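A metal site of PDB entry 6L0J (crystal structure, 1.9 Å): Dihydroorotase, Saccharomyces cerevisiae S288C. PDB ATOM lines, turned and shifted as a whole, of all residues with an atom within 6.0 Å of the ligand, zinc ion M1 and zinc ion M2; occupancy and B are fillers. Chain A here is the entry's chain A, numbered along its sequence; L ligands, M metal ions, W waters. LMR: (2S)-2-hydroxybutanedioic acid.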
ATOM      1  N   HIS A  14       4.718  -0.368  12.686  1.00  0.00           N
ATOM      2  CA  HIS A  14       5.118  -1.151  11.503  1.00  0.00           C
ATOM      3  C   HIS A  14       6.553  -0.769  11.133  1.00  0.00           C
ATOM      4  O   HIS A  14       6.769   0.144  10.333  1.00  0.00           O
ATOM      5  CB  HIS A  14       4.152  -0.934  10.344  1.00  0.00           C
ATOM      6  CG  HIS A  14       4.330  -1.889   9.201  1.00  0.00           C
ATOM      7  ND1 HIS A  14       3.274  -2.464   8.524  1.00  0.00           N
ATOM      8  CD2 HIS A  14       5.457  -2.391   8.628  1.00  0.00           C
ATOM      9  CE1 HIS A  14       3.742  -3.267   7.576  1.00  0.00           C
ATOM     10  NE2 HIS A  14       5.064  -3.235   7.620  1.00  0.00           N
ATOM     11  N   HIS A  16      10.568  -2.099  10.077  1.00  0.00           N
ATOM     12  CA  HIS A  16      11.599  -3.049   9.659  1.00  0.00           C
ATOM     13  C   HIS A  16      12.970  -2.530  10.052  1.00  0.00           C
ATOM     14  O   HIS A  16      13.340  -1.404   9.686  1.00  0.00           O
ATOM     15  CB  HIS A  16      11.555  -3.297   8.145  1.00  0.00           C
ATOM     16  CG  HIS A  16      10.254  -3.840   7.662  1.00  0.00           C
ATOM     17  ND1 HIS A  16      10.022  -5.183   7.501  1.00  0.00           N
ATOM     18  CD2 HIS A  16       9.107  -3.207   7.300  1.00  0.00           C
ATOM     19  CE1 HIS A  16       8.787  -5.365   7.053  1.00  0.00           C
ATOM     20  NE2 HIS A  16       8.218  -4.183   6.920  1.00  0.00           N
ATOM     21  N   ARG A  18      15.765  -4.949   9.891  1.00  0.00           N
ATOM     22  CA  ARG A  18      16.693  -5.874   9.221  1.00  0.00           C
ATOM     23  C   ARG A  18      17.612  -6.520  10.280  1.00  0.00           C
ATOM     24  O   ARG A  18      17.210  -6.725  11.429  1.00  0.00           O
ATOM     25  CB  ARG A  18      17.465  -5.153   8.113  1.00  0.00           C
ATOM     26  CG  ARG A  18      16.617  -4.252   7.193  1.00  0.00           C
ATOM     27  CD  ARG A  18      15.562  -5.054   6.386  1.00  0.00           C
ATOM     28  NE  ARG A  18      14.977  -4.196   5.359  1.00  0.00           N
ATOM     29  CZ  ARG A  18      13.763  -4.347   4.841  1.00  0.00           C
ATOM     30  NH1 ARG A  18      12.966  -5.340   5.244  1.00  0.00           N
ATOM     31  NH2 ARG A  18      13.361  -3.504   3.897  1.00  0.00           N
ATOM     32  N   MET A  41       8.605  -5.991  12.512  1.00  0.00           N
ATOM     33  CA  MET A  41       8.128  -6.979  11.553  1.00  0.00           C
ATOM     34  C   MET A  41       9.128  -8.119  11.397  1.00  0.00           C
ATOM     35  O   MET A  41      10.323  -7.955  11.642  1.00  0.00           O
ATOM     36  CB  MET A  41       7.866  -6.316  10.207  1.00  0.00           C
ATOM     37  CG  MET A  41       6.633  -5.404  10.252  1.00  0.00           C
ATOM     38  SD  MET A  41       5.158  -6.358  10.772  1.00  0.00           S
ATOM     39  CE  MET A  41       3.962  -5.048  11.114  1.00  0.00           C
ATOM     40  N   ASN A  43       9.917 -10.333   8.662  1.00  0.00           N
ATOM     41  CA  ASN A  43      10.330 -10.817   7.341  1.00  0.00           C
ATOM     42  C   ASN A  43      11.851 -10.735   7.135  1.00  0.00           C
ATOM     43  O   ASN A  43      12.355 -10.131   6.174  1.00  0.00           O
ATOM     44  CB  ASN A  43       9.580 -10.062   6.253  1.00  0.00           C
ATOM     45  CG  ASN A  43       9.924  -8.577   6.221  1.00  0.00           C
ATOM     46  OD1 ASN A  43      10.251  -7.987   7.261  1.00  0.00           O
ATOM     47  ND2 ASN A  43       9.885  -7.962   5.038  1.00  0.00           N
ATOM     48  N   KCX A  98       2.510 -11.726  11.722  1.00  0.00           N
ATOM     49  CA  KCX A  98       2.323 -10.967  10.489  1.00  0.00           C
ATOM     50  CB  KCX A  98       3.508 -10.003  10.289  1.00  0.00           C
ATOM     51  CG  KCX A  98       3.585  -9.324   8.908  1.00  0.00           C
ATOM     52  CD  KCX A  98       2.481  -8.280   8.772  1.00  0.00           C
ATOM     53  CE  KCX A  98       2.686  -7.519   7.511  1.00  0.00           C
ATOM     54  NZ  KCX A  98       4.061  -6.956   7.539  1.00  0.00           N
ATOM     55  C   KCX A  98       2.193 -11.897   9.294  1.00  0.00           C
ATOM     56  O   KCX A  98       3.024 -12.790   9.085  1.00  0.00           O
ATOM     57  CX  KCX A  98       4.471  -6.150   6.561  1.00  0.00           C
ATOM     58  OQ1 KCX A  98       3.689  -5.830   5.623  1.00  0.00           O
ATOM     59  OQ2 KCX A  98       5.633  -5.706   6.607  1.00  0.00           O
ATOM     60  N   TYR A 100       2.328 -12.419   5.269  1.00  0.00           N
ATOM     61  CA  TYR A 100       2.770 -11.999   3.944  1.00  0.00           C
ATOM     62  C   TYR A 100       2.217 -12.978   2.930  1.00  0.00           C
ATOM     63  O   TYR A 100       2.627 -14.153   2.926  1.00  0.00           O
ATOM     64  CB  TYR A 100       4.302 -11.982   3.848  1.00  0.00           C
ATOM     65  CG  TYR A 100       4.960 -10.981   4.781  1.00  0.00           C
ATOM     66  CD1 TYR A 100       5.187  -9.673   4.360  1.00  0.00           C
ATOM     67  CD2 TYR A 100       5.348 -11.341   6.043  1.00  0.00           C
ATOM     68  CE1 TYR A 100       5.781  -8.749   5.204  1.00  0.00           C
ATOM     69  CE2 TYR A 100       5.961 -10.423   6.907  1.00  0.00           C
ATOM     70  CZ  TYR A 100       6.178  -9.129   6.471  1.00  0.00           C
ATOM     71  OH  TYR A 100       6.749  -8.203   7.307  1.00  0.00           O
ATOM     72  N   VAL A 104       4.361 -11.251  -2.812  1.00  0.00           N
ATOM     73  CA  VAL A 104       3.920  -9.879  -3.051  1.00  0.00           C
ATOM     74  C   VAL A 104       4.907  -8.826  -2.555  1.00  0.00           C
ATOM     75  O   VAL A 104       4.768  -7.646  -2.927  1.00  0.00           O
ATOM     76  CB  VAL A 104       2.528  -9.559  -2.448  1.00  0.00           C
ATOM     77  CG1 VAL A 104       1.471 -10.556  -2.952  1.00  0.00           C
ATOM     78  CG2 VAL A 104       2.558  -9.553  -0.925  1.00  0.00           C
ATOM     79  N   THR A 105       5.880  -9.184  -1.724  1.00  0.00           N
ATOM     80  CA  THR A 105       6.794  -8.142  -1.233  1.00  0.00           C
ATOM     81  C   THR A 105       8.099  -8.747  -0.725  1.00  0.00           C
ATOM     82  O   THR A 105       8.356  -9.946  -0.888  1.00  0.00           O
ATOM     83  CB  THR A 105       6.107  -7.299  -0.141  1.00  0.00           C
ATOM     84  OG1 THR A 105       6.930  -6.148   0.141  1.00  0.00           O
ATOM     85  CG2 THR A 105       5.879  -8.118   1.135  1.00  0.00           C
ATOM     86  N   THR A 106       8.931  -7.902  -0.122  1.00  0.00           N
ATOM     87  CA  THR A 106      10.259  -8.293   0.344  1.00  0.00           C
ATOM     88  C   THR A 106      10.207  -9.513   1.264  1.00  0.00           C
ATOM     89  O   THR A 106       9.488  -9.511   2.260  1.00  0.00           O
ATOM     90  CB  THR A 106      10.909  -7.137   1.099  1.00  0.00           C
ATOM     91  OG1 THR A 106      10.970  -5.976   0.243  1.00  0.00           O
ATOM     92  CG2 THR A 106      12.311  -7.539   1.610  1.00  0.00           C
ATOM     93  N   ASN A 107      10.984 -10.540   0.932  1.00  0.00           N
ATOM     94  CA  ASN A 107      11.127 -11.719   1.791  1.00  0.00           C
ATOM     95  C   ASN A 107       9.785 -12.387   2.047  1.00  0.00           C
ATOM     96  O   ASN A 107       9.498 -12.824   3.166  1.00  0.00           O
ATOM     97  CB  ASN A 107      11.812 -11.360   3.116  1.00  0.00           C
ATOM     98  CG  ASN A 107      13.266 -10.954   2.951  1.00  0.00           C
ATOM     99  OD1 ASN A 107      13.881 -11.250   1.933  1.00  0.00           O
ATOM    100  ND2 ASN A 107      13.831 -10.268   3.944  1.00  0.00           N
ATOM    101  N   HIS A 137      -0.388  -8.003   5.543  1.00  0.00           N
ATOM    102  CA  HIS A 137      -0.020  -7.327   4.285  1.00  0.00           C
ATOM    103  C   HIS A 137      -1.099  -7.738   3.289  1.00  0.00           C
ATOM    104  O   HIS A 137      -1.032  -8.786   2.647  1.00  0.00           O
ATOM    105  CB  HIS A 137       1.385  -7.708   3.800  1.00  0.00           C
ATOM    106  CG  HIS A 137       1.799  -7.009   2.526  1.00  0.00           C
ATOM    107  ND1 HIS A 137       2.857  -6.118   2.463  1.00  0.00           N
ATOM    108  CD2 HIS A 137       1.263  -7.041   1.277  1.00  0.00           C
ATOM    109  CE1 HIS A 137       2.952  -5.633   1.230  1.00  0.00           C
ATOM    110  NE2 HIS A 137       1.998  -6.186   0.493  1.00  0.00           N
ATOM    111  N   GLU A 179      -2.429  -3.648   7.412  1.00  0.00           N
ATOM    112  CA  GLU A 179      -1.254  -2.803   7.455  1.00  0.00           C
ATOM    113  C   GLU A 179      -1.237  -1.882   6.242  1.00  0.00           C
ATOM    114  O   GLU A 179      -1.789  -2.190   5.200  1.00  0.00           O
ATOM    115  CB  GLU A 179       0.033  -3.657   7.443  1.00  0.00           C
ATOM    116  CG  GLU A 179       0.258  -4.494   8.699  1.00  0.00           C
ATOM    117  CD  GLU A 179       0.373  -3.647   9.983  1.00  0.00           C
ATOM    118  OE1 GLU A 179       0.745  -2.458   9.896  1.00  0.00           O
ATOM    119  OE2 GLU A 179       0.077  -4.165  11.069  1.00  0.00           O
ATOM    120  N   HIS A 180      -0.532  -0.755   6.391  1.00  0.00           N
ATOM    121  CA  HIS A 180      -0.263   0.215   5.332  1.00  0.00           C
ATOM    122  C   HIS A 180      -1.324   0.275   4.229  1.00  0.00           C
ATOM    123  O   HIS A 180      -1.087  -0.157   3.093  1.00  0.00           O
ATOM    124  CB  HIS A 180       1.145  -0.020   4.726  1.00  0.00           C
ATOM    125  CG  HIS A 180       1.482  -1.453   4.388  1.00  0.00           C
ATOM    126  ND1 HIS A 180       0.612  -2.343   3.799  1.00  0.00           N
ATOM    127  CD2 HIS A 180       2.663  -2.129   4.512  1.00  0.00           C
ATOM    128  CE1 HIS A 180       1.219  -3.499   3.589  1.00  0.00           C
ATOM    129  NE2 HIS A 180       2.469  -3.397   4.021  1.00  0.00           N
ATOM    130  N   CYS A 229       7.539   1.033  -3.320  1.00  0.00           N
ATOM    131  CA  CYS A 229       7.261   0.213  -2.154  1.00  0.00           C
ATOM    132  C   CYS A 229       6.078  -0.676  -2.504  1.00  0.00           C
ATOM    133  O   CYS A 229       5.459  -0.541  -3.573  1.00  0.00           O
ATOM    134  CB  CYS A 229       6.994   1.075  -0.905  1.00  0.00           C
ATOM    135  SG  CYS A 229       5.491   2.157  -1.006  1.00  0.00           S
ATOM    136  N   LYS A 230       5.794  -1.645  -1.627  1.00  0.00           N
ATOM    137  CA  LYS A 230       4.560  -2.417  -1.654  1.00  0.00           C
ATOM    138  C   LYS A 230       3.774  -2.149  -0.379  1.00  0.00           C
ATOM    139  O   LYS A 230       4.368  -2.055   0.706  1.00  0.00           O
ATOM    140  CB  LYS A 230       4.827  -3.935  -1.784  1.00  0.00           C
ATOM    141  CG  LYS A 230       5.522  -4.369  -3.088  1.00  0.00           C
ATOM    142  CD  LYS A 230       4.833  -3.860  -4.375  1.00  0.00           C
ATOM    143  CE  LYS A 230       3.486  -4.500  -4.606  1.00  0.00           C
ATOM    144  NZ  LYS A 230       3.624  -5.954  -4.932  1.00  0.00           N
ATOM    145  N   PRO A 231       2.427  -1.980  -0.463  1.00  0.00           N
ATOM    146  CA  PRO A 231       1.669  -1.885  -1.699  1.00  0.00           C
ATOM    147  C   PRO A 231       2.082  -0.579  -2.380  1.00  0.00           C
ATOM    148  O   PRO A 231       2.502   0.317  -1.658  1.00  0.00           O
ATOM    149  CB  PRO A 231       0.176  -1.842  -1.243  1.00  0.00           C
ATOM    150  CG  PRO A 231       0.218  -2.146   0.255  1.00  0.00           C
ATOM    151  CD  PRO A 231       1.594  -1.706   0.721  1.00  0.00           C
ATOM    152  N   ASP A 258       5.976   1.526   8.080  1.00  0.00           N
ATOM    153  CA  ASP A 258       6.601   0.611   7.124  1.00  0.00           C
ATOM    154  C   ASP A 258       7.932   1.183   6.646  1.00  0.00           C
ATOM    155  O   ASP A 258       8.274   1.052   5.463  1.00  0.00           O
ATOM    156  CB  ASP A 258       5.712   0.305   5.913  1.00  0.00           C
ATOM    157  CG  ASP A 258       6.168  -0.952   5.140  1.00  0.00           C
ATOM    158  OD1 ASP A 258       6.818  -1.823   5.769  1.00  0.00           O
ATOM    159  OD2 ASP A 258       5.916  -1.074   3.918  1.00  0.00           O
ATOM    160  N   SER A 259       8.716   1.774   7.550  1.00  0.00           N
ATOM    161  CA  SER A 259      10.070   2.132   7.161  1.00  0.00           C
ATOM    162  C   SER A 259      10.814   0.852   6.811  1.00  0.00           C
ATOM    163  O   SER A 259      10.889  -0.068   7.616  1.00  0.00           O
ATOM    164  CB  SER A 259      10.784   2.894   8.272  1.00  0.00           C
ATOM    165  OG  SER A 259      12.117   3.190   7.867  1.00  0.00           O
ATOM    166  N   ALA A 260      11.302   0.781   5.579  1.00  0.00           N
ATOM    167  CA  ALA A 260      11.777  -0.473   4.975  1.00  0.00           C
ATOM    168  C   ALA A 260      13.138  -0.211   4.339  1.00  0.00           C
ATOM    169  O   ALA A 260      13.238   0.027   3.134  1.00  0.00           O
ATOM    170  CB  ALA A 260      10.797  -0.993   3.937  1.00  0.00           C
ATOM    171  N   PRO A 261      14.201  -0.253   5.131  1.00  0.00           N
ATOM    172  CA  PRO A 261      15.502   0.177   4.604  1.00  0.00           C
ATOM    173  C   PRO A 261      16.154  -0.843   3.683  1.00  0.00           C
ATOM    174  O   PRO A 261      16.147  -2.049   3.928  1.00  0.00           O
ATOM    175  CB  PRO A 261      16.343   0.401   5.877  1.00  0.00           C
ATOM    176  CG  PRO A 261      15.679  -0.355   6.935  1.00  0.00           C
ATOM    177  CD  PRO A 261      14.212  -0.408   6.588  1.00  0.00           C
ATOM    178  N   HIS A 262      16.708  -0.327   2.584  1.00  0.00           N
ATOM    179  CA  HIS A 262      17.500  -1.079   1.644  1.00  0.00           C
ATOM    180  C   HIS A 262      18.738  -0.264   1.307  1.00  0.00           C
ATOM    181  O   HIS A 262      18.652   0.963   1.212  1.00  0.00           O
ATOM    182  CB  HIS A 262      16.735  -1.359   0.336  1.00  0.00           C
ATOM    183  CG  HIS A 262      15.532  -2.221   0.511  1.00  0.00           C
ATOM    184  ND1 HIS A 262      15.612  -3.587   0.682  1.00  0.00           N
ATOM    185  CD2 HIS A 262      14.213  -1.918   0.534  1.00  0.00           C
ATOM    186  CE1 HIS A 262      14.395  -4.089   0.810  1.00  0.00           C
ATOM    187  NE2 HIS A 262      13.530  -3.091   0.735  1.00  0.00           N
ATOM    188  N   ALA A 275      11.513  -3.392  -3.012  1.00  0.00           N
ATOM    189  CA  ALA A 275      10.395  -2.567  -2.596  1.00  0.00           C
ATOM    190  C   ALA A 275      10.641  -2.052  -1.187  1.00  0.00           C
ATOM    191  O   ALA A 275      10.998  -2.831  -0.302  1.00  0.00           O
ATOM    192  CB  ALA A 275       9.103  -3.366  -2.635  1.00  0.00           C
ATOM    193  N   GLY A 276      10.421  -0.763  -0.956  1.00  0.00           N
ATOM    194  CA  GLY A 276      10.589  -0.227   0.394  1.00  0.00           C
ATOM    195  C   GLY A 276      11.091   1.211   0.449  1.00  0.00           C
ATOM    196  O   GLY A 276      12.016   1.591  -0.274  1.00  0.00           O
HETATM  197  C1  LMR L   1       6.673  -4.502   2.998  1.00  0.00           C
HETATM  198  O1A LMR L   1       6.116  -4.127   4.072  1.00  0.00           O
HETATM  199  O1B LMR L   1       5.919  -4.898   2.079  1.00  0.00           O
HETATM  200  C2  LMR L   1       8.198  -4.572   2.731  1.00  0.00           C
HETATM  201  O2  LMR L   1       8.733  -3.787   1.651  1.00  0.00           O
HETATM  202  C3  LMR L   1       8.984  -4.111   3.901  1.00  0.00           C
HETATM  203  C4  LMR L   1      10.336  -4.729   3.559  1.00  0.00           C
HETATM  204  O4A LMR L   1      11.057  -4.323   2.581  1.00  0.00           O
HETATM  205  O4B LMR L   1      10.648  -5.669   4.286  1.00  0.00           O
HETATM  206 ZN    ZN M   1       3.824  -4.977   3.862  1.00  0.00          ZN
HETATM  207 ZN    ZN M   2       6.306  -3.786   6.133  1.00  0.00          ZN
HETATM  208  O   HOH W   1       6.999  -1.586   1.207  1.00  0.00           O
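Zinc ion M1 is bound by OQ1 of KCX 98 (2.0 Å), ND1 of His 137 (2.0 Å), NE2 of His 180 (2.1 Å) and O1A of the ligand (2.5 Å). Zinc ion M1 has four donor atoms within binding distance. Slightly farther from zinc ion M1 lies an oxygen (O1B) of the ligand (2.8 Å).
O of Lys 230 touches O1B of the ligand, 3.5 Å away. CB of Ala 260 touches O4A of the ligand (3.6 Å). The nearest printed residue that does not touch the ligand is Gly 276 (4.2 Å).
The side-chain hydroxyl of Thr 105 lies within hydrogen-bond range of an oxygen (O1B) of the ligand (2.5 Å). NH1 of Arg 18 is in salt-bridge range of O4B of the ligand (2.5 Å). The side-chain amide nitrogen of Asn 43 lies within hydrogen-bond range of an oxygen (O4B) of the ligand (2.5 Å). An oxygen (O4A) of the ligand lies within hydrogen-bond range of the side-chain hydroxyl (OG1) of Thr 106 (2.9 Å). An oxygen (O2) of the ligand sits at hydrogen-bond distance from the backbone carbonyl oxygen (O) of Ala 275 (3.1 Å). O4A of the ligand is in hydrogen-bond range of NE2 of His 262, at 3.3 Å.
Zinc ion M2 is bound by a ring nitrogen (NE2) of His 14 (2.0 Å), the side-chain carboxylate of Asp 258 (2.1 Å), OQ2 of KCX 98 (2.1 Å), an oxygen (O1A) of the ligand (2.1 Å) and a ring nitrogen (NE2) of His 16 (2.1 Å). Zinc ion M2 has five donor atoms within binding distance.
NZ of KCX 98 is in hydrogen-bond range of OH of Tyr 100 (3.0 Å). A ring nitrogen (ND1) of His 16 is in hydrogen-bond range of the side-chain amide oxygen (OD1) of Asn 43, 2.8 Å away. The backbone carbonyl oxygen (O) of Ser 259 is in hydrogen-bond range of the backbone NH (N) of His 16 (3.2 Å). A ring nitrogen (NE2) of His 262 is in hydrogen-bond range of the guanidinium group of Arg 18, 3.2 Å away. The guanidinium group (NE) of Arg 18 is in hydrogen-bond range of the backbone carbonyl oxygen (O) of Pro 261 (2.8 Å). The side-chain amide nitrogen (ND2) of Asn 43 is in hydrogen-bond range of the backbone carbonyl oxygen (O) of Thr 106 (3.2 Å). O of Asn 43 is in hydrogen-bond range of ND2 of Asn 107 (2.7 Å). The side-chain hydroxyl (OG1) of Thr 106 is in hydrogen-bond range of the backbone carbonyl oxygen (O) of Ala 275, 3.2 Å away.
Water W1 lies within hydrogen-bond range of O of Lys 230 (2.7 Å), O2 of the ligand (2.8 Å) and OD2 of Asp 258 (3.0 Å).
Four residues have an atom within 4 Å of zinc ion M2: His 14, His 16, KCX 98 and Asp 258. The nearest printed residue that does not touch zinc ion M2 is His 180 (4.3 Å).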
